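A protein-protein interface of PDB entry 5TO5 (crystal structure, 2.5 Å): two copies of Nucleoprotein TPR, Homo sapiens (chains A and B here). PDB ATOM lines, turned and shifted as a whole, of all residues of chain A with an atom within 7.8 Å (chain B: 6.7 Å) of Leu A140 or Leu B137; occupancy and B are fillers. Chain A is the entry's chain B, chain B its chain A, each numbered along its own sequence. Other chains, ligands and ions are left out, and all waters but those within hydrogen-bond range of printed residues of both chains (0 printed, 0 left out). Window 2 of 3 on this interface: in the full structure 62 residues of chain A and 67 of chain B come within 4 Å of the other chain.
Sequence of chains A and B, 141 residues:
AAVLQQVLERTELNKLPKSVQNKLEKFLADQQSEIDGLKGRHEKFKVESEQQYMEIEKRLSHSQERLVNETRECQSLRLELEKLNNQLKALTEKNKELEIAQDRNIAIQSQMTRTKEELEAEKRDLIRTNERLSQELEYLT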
ATOM      1  N   ARG A 132     -27.433  13.921   4.142  1.00  0.00           N
ATOM      2  CA  ARG A 132     -27.782  15.188   4.775  1.00  0.00           C
ATOM      3  C   ARG A 132     -27.487  15.158   6.274  1.00  0.00           C
ATOM      4  O   ARG A 132     -26.939  16.111   6.828  1.00  0.00           O
ATOM      5  CB  ARG A 132     -29.257  15.509   4.515  1.00  0.00           C
ATOM      6  CG  ARG A 132     -29.897  16.488   5.488  1.00  0.00           C
ATOM      7  CD  ARG A 132     -29.283  17.881   5.406  1.00  0.00           C
ATOM      8  NE  ARG A 132     -30.200  18.901   5.908  1.00  0.00           N
ATOM      9  CZ  ARG A 132     -29.823  20.002   6.548  1.00  0.00           C
ATOM     10  NH1 ARG A 132     -28.542  20.229   6.781  1.00  0.00           N
ATOM     11  NH2 ARG A 132     -30.732  20.871   6.960  1.00  0.00           N
ATOM     12  N   LEU A 133     -27.843  14.052   6.921  1.00  0.00           N
ATOM     13  CA  LEU A 133     -27.577  13.869   8.344  1.00  0.00           C
ATOM     14  C   LEU A 133     -26.086  13.812   8.652  1.00  0.00           C
ATOM     15  O   LEU A 133     -25.647  14.263   9.710  1.00  0.00           O
ATOM     16  CB  LEU A 133     -28.251  12.595   8.854  1.00  0.00           C
ATOM     17  CG  LEU A 133     -29.772  12.633   8.990  1.00  0.00           C
ATOM     18  CD1 LEU A 133     -30.301  11.254   9.321  1.00  0.00           C
ATOM     19  CD2 LEU A 133     -30.188  13.641  10.045  1.00  0.00           C
ATOM     20  N   SER A 134     -25.311  13.243   7.737  1.00  0.00           N
ATOM     21  CA  SER A 134     -23.875  13.122   7.942  1.00  0.00           C
ATOM     22  C   SER A 134     -23.205  14.488   7.914  1.00  0.00           C
ATOM     23  O   SER A 134     -22.418  14.822   8.800  1.00  0.00           O
ATOM     24  CB  SER A 134     -23.257  12.206   6.886  1.00  0.00           C
ATOM     25  OG  SER A 134     -23.761  10.886   7.009  1.00  0.00           O
ATOM     26  N   GLN A 135     -23.536  15.287   6.904  1.00  0.00           N
ATOM     27  CA  GLN A 135     -22.915  16.594   6.753  1.00  0.00           C
ATOM     28  C   GLN A 135     -23.336  17.520   7.892  1.00  0.00           C
ATOM     29  O   GLN A 135     -22.626  18.472   8.222  1.00  0.00           O
ATOM     30  CB  GLN A 135     -23.263  17.211   5.395  1.00  0.00           C
ATOM     31  CG  GLN A 135     -24.577  17.972   5.343  1.00  0.00           C
ATOM     32  CD  GLN A 135     -24.585  19.008   4.236  1.00  0.00           C
ATOM     33  OE1 GLN A 135     -23.952  18.828   3.194  1.00  0.00           O
ATOM     34  NE2 GLN A 135     -25.292  20.109   4.462  1.00  0.00           N
ATOM     35  N   GLU A 136     -24.476  17.226   8.507  1.00  0.00           N
ATOM     36  CA  GLU A 136     -24.943  18.029   9.628  1.00  0.00           C
ATOM     37  C   GLU A 136     -24.168  17.682  10.891  1.00  0.00           C
ATOM     38  O   GLU A 136     -23.932  18.538  11.743  1.00  0.00           O
ATOM     39  CB  GLU A 136     -26.439  17.832   9.850  1.00  0.00           C
ATOM     40  CG  GLU A 136     -27.076  18.966  10.620  1.00  0.00           C
ATOM     41  CD  GLU A 136     -26.894  20.298   9.923  1.00  0.00           C
ATOM     42  OE1 GLU A 136     -26.726  21.320  10.620  1.00  0.00           O
ATOM     43  OE2 GLU A 136     -26.921  20.321   8.674  1.00  0.00           O
ATOM     44  N   LEU A 137     -23.786  16.415  11.010  1.00  0.00           N
ATOM     45  CA  LEU A 137     -22.935  15.979  12.107  1.00  0.00           C
ATOM     46  C   LEU A 137     -21.555  16.615  11.995  1.00  0.00           C
ATOM     47  O   LEU A 137     -21.001  17.093  12.982  1.00  0.00           O
ATOM     48  CB  LEU A 137     -22.825  14.452  12.127  1.00  0.00           C
ATOM     49  CG  LEU A 137     -23.974  13.731  12.836  1.00  0.00           C
ATOM     50  CD1 LEU A 137     -23.897  12.229  12.610  1.00  0.00           C
ATOM     51  CD2 LEU A 137     -23.952  14.054  14.321  1.00  0.00           C
ATOM     52  N   GLU A 138     -21.013  16.621  10.782  1.00  0.00           N
ATOM     53  CA  GLU A 138     -19.717  17.237  10.499  1.00  0.00           C
ATOM     54  C   GLU A 138     -19.667  18.688  10.972  1.00  0.00           C
ATOM     55  O   GLU A 138     -18.711  19.120  11.613  1.00  0.00           O
ATOM     56  CB  GLU A 138     -19.423  17.161   8.997  1.00  0.00           C
ATOM     57  CG  GLU A 138     -18.173  17.896   8.558  1.00  0.00           C
ATOM     58  CD  GLU A 138     -16.904  17.162   8.936  1.00  0.00           C
ATOM     59  OE1 GLU A 138     -16.991  15.964   9.281  1.00  0.00           O
ATOM     60  OE2 GLU A 138     -15.820  17.779   8.885  1.00  0.00           O
ATOM     61  N   TYR A 139     -20.727  19.420  10.655  1.00  0.00           N
ATOM     62  CA  TYR A 139     -20.888  20.820  11.032  1.00  0.00           C
ATOM     63  C   TYR A 139     -20.893  21.027  12.542  1.00  0.00           C
ATOM     64  O   TYR A 139     -20.344  22.010  13.048  1.00  0.00           O
ATOM     65  CB  TYR A 139     -22.187  21.356  10.428  1.00  0.00           C
ATOM     66  CG  TYR A 139     -22.519  22.780  10.775  1.00  0.00           C
ATOM     67  CD1 TYR A 139     -21.927  23.839  10.102  1.00  0.00           C
ATOM     68  CD2 TYR A 139     -23.450  23.066  11.763  1.00  0.00           C
ATOM     69  CE1 TYR A 139     -22.239  25.149  10.418  1.00  0.00           C
ATOM     70  CE2 TYR A 139     -23.773  24.368  12.084  1.00  0.00           C
ATOM     71  CZ  TYR A 139     -23.164  25.405  11.408  1.00  0.00           C
ATOM     72  OH  TYR A 139     -23.486  26.700  11.726  1.00  0.00           O
ATOM     73  N   LEU A 140     -21.518  20.096  13.256  1.00  0.00           N
ATOM     74  CA  LEU A 140     -21.676  20.214  14.700  1.00  0.00           C
ATOM     75  C   LEU A 140     -20.510  19.615  15.486  1.00  0.00           C
ATOM     76  O   LEU A 140     -20.406  19.821  16.695  1.00  0.00           O
ATOM     77  CB  LEU A 140     -22.984  19.554  15.138  1.00  0.00           C
ATOM     78  CG  LEU A 140     -24.277  20.170  14.601  1.00  0.00           C
ATOM     79  CD1 LEU A 140     -25.475  19.459  15.187  1.00  0.00           C
ATOM     80  CD2 LEU A 140     -24.341  21.655  14.907  1.00  0.00           C
ATOM     81  N   THR A 141     -19.639  18.874  14.807  1.00  0.00           N
ATOM     82  CA  THR A 141     -18.462  18.307  15.461  1.00  0.00           C
ATOM     83  C   THR A 141     -17.388  17.941  14.444  1.00  0.00           C
ATOM     84  O   THR A 141     -16.770  18.818  13.841  1.00  0.00           O
ATOM     85  CB  THR A 141     -18.818  17.055  16.300  1.00  0.00           C
ATOM     86  OG1 THR A 141     -17.647  16.571  16.968  1.00  0.00           O
ATOM     87  CG2 THR A 141     -19.387  15.952  15.421  1.00  0.00           C
ATOM     88  N   ARG B 132     -29.345   5.837  13.977  1.00  0.00           N
ATOM     89  CA  ARG B 132     -28.109   6.017  14.738  1.00  0.00           C
ATOM     90  C   ARG B 132     -27.555   7.434  14.574  1.00  0.00           C
ATOM     91  O   ARG B 132     -27.092   8.044  15.540  1.00  0.00           O
ATOM     92  CB  ARG B 132     -27.052   4.993  14.319  1.00  0.00           C
ATOM     93  CG  ARG B 132     -25.686   5.258  14.931  1.00  0.00           C
ATOM     94  CD  ARG B 132     -24.704   4.133  14.659  1.00  0.00           C
ATOM     95  NE  ARG B 132     -24.547   3.860  13.234  1.00  0.00           N
ATOM     96  CZ  ARG B 132     -23.809   4.593  12.408  1.00  0.00           C
ATOM     97  NH1 ARG B 132     -23.161   5.661  12.854  1.00  0.00           N
ATOM     98  NH2 ARG B 132     -23.725   4.263  11.128  1.00  0.00           N
ATOM     99  N   LEU B 133     -27.606   7.952  13.350  1.00  0.00           N
ATOM    100  CA  LEU B 133     -27.158   9.316  13.076  1.00  0.00           C
ATOM    101  C   LEU B 133     -28.124  10.331  13.680  1.00  0.00           C
ATOM    102  O   LEU B 133     -27.717  11.410  14.109  1.00  0.00           O
ATOM    103  CB  LEU B 133     -27.023   9.554  11.567  1.00  0.00           C
ATOM    104  CG  LEU B 133     -26.002   8.762  10.741  1.00  0.00           C
ATOM    105  CD1 LEU B 133     -26.043   9.232   9.295  1.00  0.00           C
ATOM    106  CD2 LEU B 133     -24.594   8.891  11.303  1.00  0.00           C
ATOM    107  N   SER B 134     -29.406   9.973  13.701  1.00  0.00           N
ATOM    108  CA  SER B 134     -30.434  10.814  14.303  1.00  0.00           C
ATOM    109  C   SER B 134     -30.174  10.985  15.794  1.00  0.00           C
ATOM    110  O   SER B 134     -30.269  12.089  16.330  1.00  0.00           O
ATOM    111  CB  SER B 134     -31.824  10.215  14.086  1.00  0.00           C
ATOM    112  OG  SER B 134     -32.113  10.085  12.709  1.00  0.00           O
ATOM    113  N   GLN B 135     -29.844   9.879  16.453  1.00  0.00           N
ATOM    114  CA  GLN B 135     -29.563   9.876  17.884  1.00  0.00           C
ATOM    115  C   GLN B 135     -28.275  10.631  18.216  1.00  0.00           C
ATOM    116  O   GLN B 135     -28.212  11.347  19.215  1.00  0.00           O
ATOM    117  CB  GLN B 135     -29.485   8.436  18.401  1.00  0.00           C
ATOM    118  CG  GLN B 135     -29.033   8.295  19.846  1.00  0.00           C
ATOM    119  CD  GLN B 135     -29.970   8.975  20.829  1.00  0.00           C
ATOM    120  OE1 GLN B 135     -31.186   8.780  20.790  1.00  0.00           O
ATOM    121  NE2 GLN B 135     -29.401   9.777  21.722  1.00  0.00           N
ATOM    122  N   GLU B 136     -27.252  10.475  17.379  1.00  0.00           N
ATOM    123  CA  GLU B 136     -25.992  11.188  17.582  1.00  0.00           C
ATOM    124  C   GLU B 136     -26.195  12.684  17.402  1.00  0.00           C
ATOM    125  O   GLU B 136     -25.443  13.500  17.937  1.00  0.00           O
ATOM    126  CB  GLU B 136     -24.918  10.686  16.618  1.00  0.00           C
ATOM    127  CG  GLU B 136     -24.242   9.393  17.048  1.00  0.00           C
ATOM    128  CD  GLU B 136     -23.534   8.708  15.901  1.00  0.00           C
ATOM    129  OE1 GLU B 136     -23.549   9.263  14.783  1.00  0.00           O
ATOM    130  OE2 GLU B 136     -22.969   7.616  16.112  1.00  0.00           O
ATOM    131  N   LEU B 137     -27.226  13.032  16.642  1.00  0.00           N
ATOM    132  CA  LEU B 137     -27.582  14.424  16.428  1.00  0.00           C
ATOM    133  C   LEU B 137     -28.294  15.020  17.637  1.00  0.00           C
ATOM    134  O   LEU B 137     -28.306  16.234  17.815  1.00  0.00           O
ATOM    135  CB  LEU B 137     -28.461  14.565  15.185  1.00  0.00           C
ATOM    136  CG  LEU B 137     -27.774  15.177  13.968  1.00  0.00           C
ATOM    137  CD1 LEU B 137     -28.784  15.479  12.878  1.00  0.00           C
ATOM    138  CD2 LEU B 137     -27.046  16.435  14.384  1.00  0.00           C
ATOM    139  N   GLU B 138     -28.894  14.167  18.461  1.00  0.00           N
ATOM    140  CA  GLU B 138     -29.635  14.649  19.620  1.00  0.00           C
ATOM    141  C   GLU B 138     -28.716  14.987  20.792  1.00  0.00           C
ATOM    142  O   GLU B 138     -29.097  15.748  21.686  1.00  0.00           O
ATOM    143  CB  GLU B 138     -30.689  13.622  20.042  1.00  0.00           C
ATOM    144  CG  GLU B 138     -31.768  13.424  18.989  1.00  0.00           C
ATOM    145  CD  GLU B 138     -33.015  12.764  19.534  1.00  0.00           C
ATOM    146  OE1 GLU B 138     -32.889  11.814  20.334  1.00  0.00           O
ATOM    147  OE2 GLU B 138     -34.123  13.198  19.159  1.00  0.00           O
ATOM    148  N   TYR B 139     -27.509  14.431  20.781  1.00  0.00           N
ATOM    149  CA  TYR B 139     -26.494  14.775  21.774  1.00  0.00           C
ATOM    150  C   TYR B 139     -25.929  16.163  21.514  1.00  0.00           C
ATOM    151  O   TYR B 139     -25.678  16.935  22.439  1.00  0.00           O
ATOM    152  CB  TYR B 139     -25.355  13.757  21.759  1.00  0.00           C
ATOM    153  CG  TYR B 139     -25.745  12.370  22.199  1.00  0.00           C
ATOM    154  CD1 TYR B 139     -26.537  12.172  23.323  1.00  0.00           C
ATOM    155  CD2 TYR B 139     -25.322  11.253  21.489  1.00  0.00           C
ATOM    156  CE1 TYR B 139     -26.895  10.901  23.727  1.00  0.00           C
ATOM    157  CE2 TYR B 139     -25.676   9.978  21.887  1.00  0.00           C
ATOM    158  CZ  TYR B 139     -26.462   9.808  23.006  1.00  0.00           C
ATOM    159  OH  TYR B 139     -26.816   8.540  23.407  1.00  0.00           O
ATOM    160  N   LEU B 140     -25.730  16.469  20.238  1.00  0.00           N
ATOM    161  CA  LEU B 140     -25.036  17.683  19.835  1.00  0.00           C
ATOM    162  C   LEU B 140     -25.974  18.885  19.737  1.00  0.00           C
ATOM    163  O   LEU B 140     -25.562  19.965  19.318  1.00  0.00           O
ATOM    164  CB  LEU B 140     -24.312  17.454  18.507  1.00  0.00           C
ATOM    165  CG  LEU B 140     -23.337  16.272  18.541  1.00  0.00           C
ATOM    166  CD1 LEU B 140     -22.656  16.087  17.200  1.00  0.00           C
ATOM    167  CD2 LEU B 140     -22.299  16.453  19.643  1.00  0.00           C
ATOM    168  N   THR B 141     -27.237  18.693  20.102  1.00  0.00           N
ATOM    169  CA  THR B 141     -28.162  19.816  20.233  1.00  0.00           C
ATOM    170  C   THR B 141     -28.754  19.885  21.638  1.00  0.00           C
ATOM    171  O   THR B 141     -28.594  18.963  22.439  1.00  0.00           O
ATOM    172  CB  THR B 141     -29.315  19.738  19.219  1.00  0.00           C
ATOM    173  OG1 THR B 141     -30.128  18.590  19.496  1.00  0.00           O
ATOM    174  CG2 THR B 141     -28.776  19.658  17.798  1.00  0.00           C
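The guanidinium group (NH1) of Arg B132 is in salt-bridge range of the side-chain carboxylate (OE2) of Glu B136, at 3.8 Å.
The backbone carbonyl oxygen (O) of Leu B137 sits at hydrogen-bond distance from the side-chain hydroxyl (OG1) of Thr B141, 3.4 Å away.
CD1 of Leu B137 touches CD2 of Leu A133, at 3.7 Å.
Ser A134 touches Leu B133.
Leu A137 touches Leu B133.
Leu A137 touches Glu B136.
Leu A137 touches Leu B137 (CD2 to CD2, 3.9 Å).
CD2 of Leu A137 touches CD1 of Leu B140, 3.8 Å away.
CD2 of Leu B137 touches CD1 of Leu A140, 3.5 Å away.
Leu B140 touches Thr A141 (CD1 to CG2, 3.7 Å).
Of the printed residues of chain B, Leu A133 touches Leu B137 (3.7 Å).
Printed residues of chain B within 4 Å of Leu A140: Leu B137.
Printed residues of chain B within 4 Å of Thr A141: Leu B140 (3.7 Å).
Printed residues of chain A within 4 Å of Leu B133: Ser A134 and Leu A137.
Of the printed residues of chain A, Glu B136 touches Leu A137.
Of the printed residues of chain A, Leu B140 touches Leu A137 and Thr A141.
Of the 10 printed residues of chain A, 5 touch a printed residue of chain B.
Along chain A the printed residues that touch a printed residue of chain B span positions 133 to 141.
Printed residues of chain B that touch a printed residue of chain A: Leu B133, Glu B136, Leu B137 and Leu B140.
Hydrophobic or aromatic side chains of chain B that line the printed part of chain A: Leu B133, Leu B137 and Leu B140.
Ser A134 touches Leu B133, but with the chains exchanged Leu A133 does not touch Ser B134 (4.02 Å).
Leu A137 touches Glu B136, but with the chains exchanged Glu A136 does not touch Leu B137 (4.5 Å).
Leu A137 touches its own counterpart, Leu B137.
Thr A141 touches Leu B140, but with the chains exchanged Leu A140 does not touch Thr B141 (4.2 Å).
Positions printed for both chains: 132, 133, 134, 135, 136, 137, 138, 139, 140 and 141.
Of the 8 pairs that touch across the chains among the printed residues, 5 have their exchanged pair printed and touching as well.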
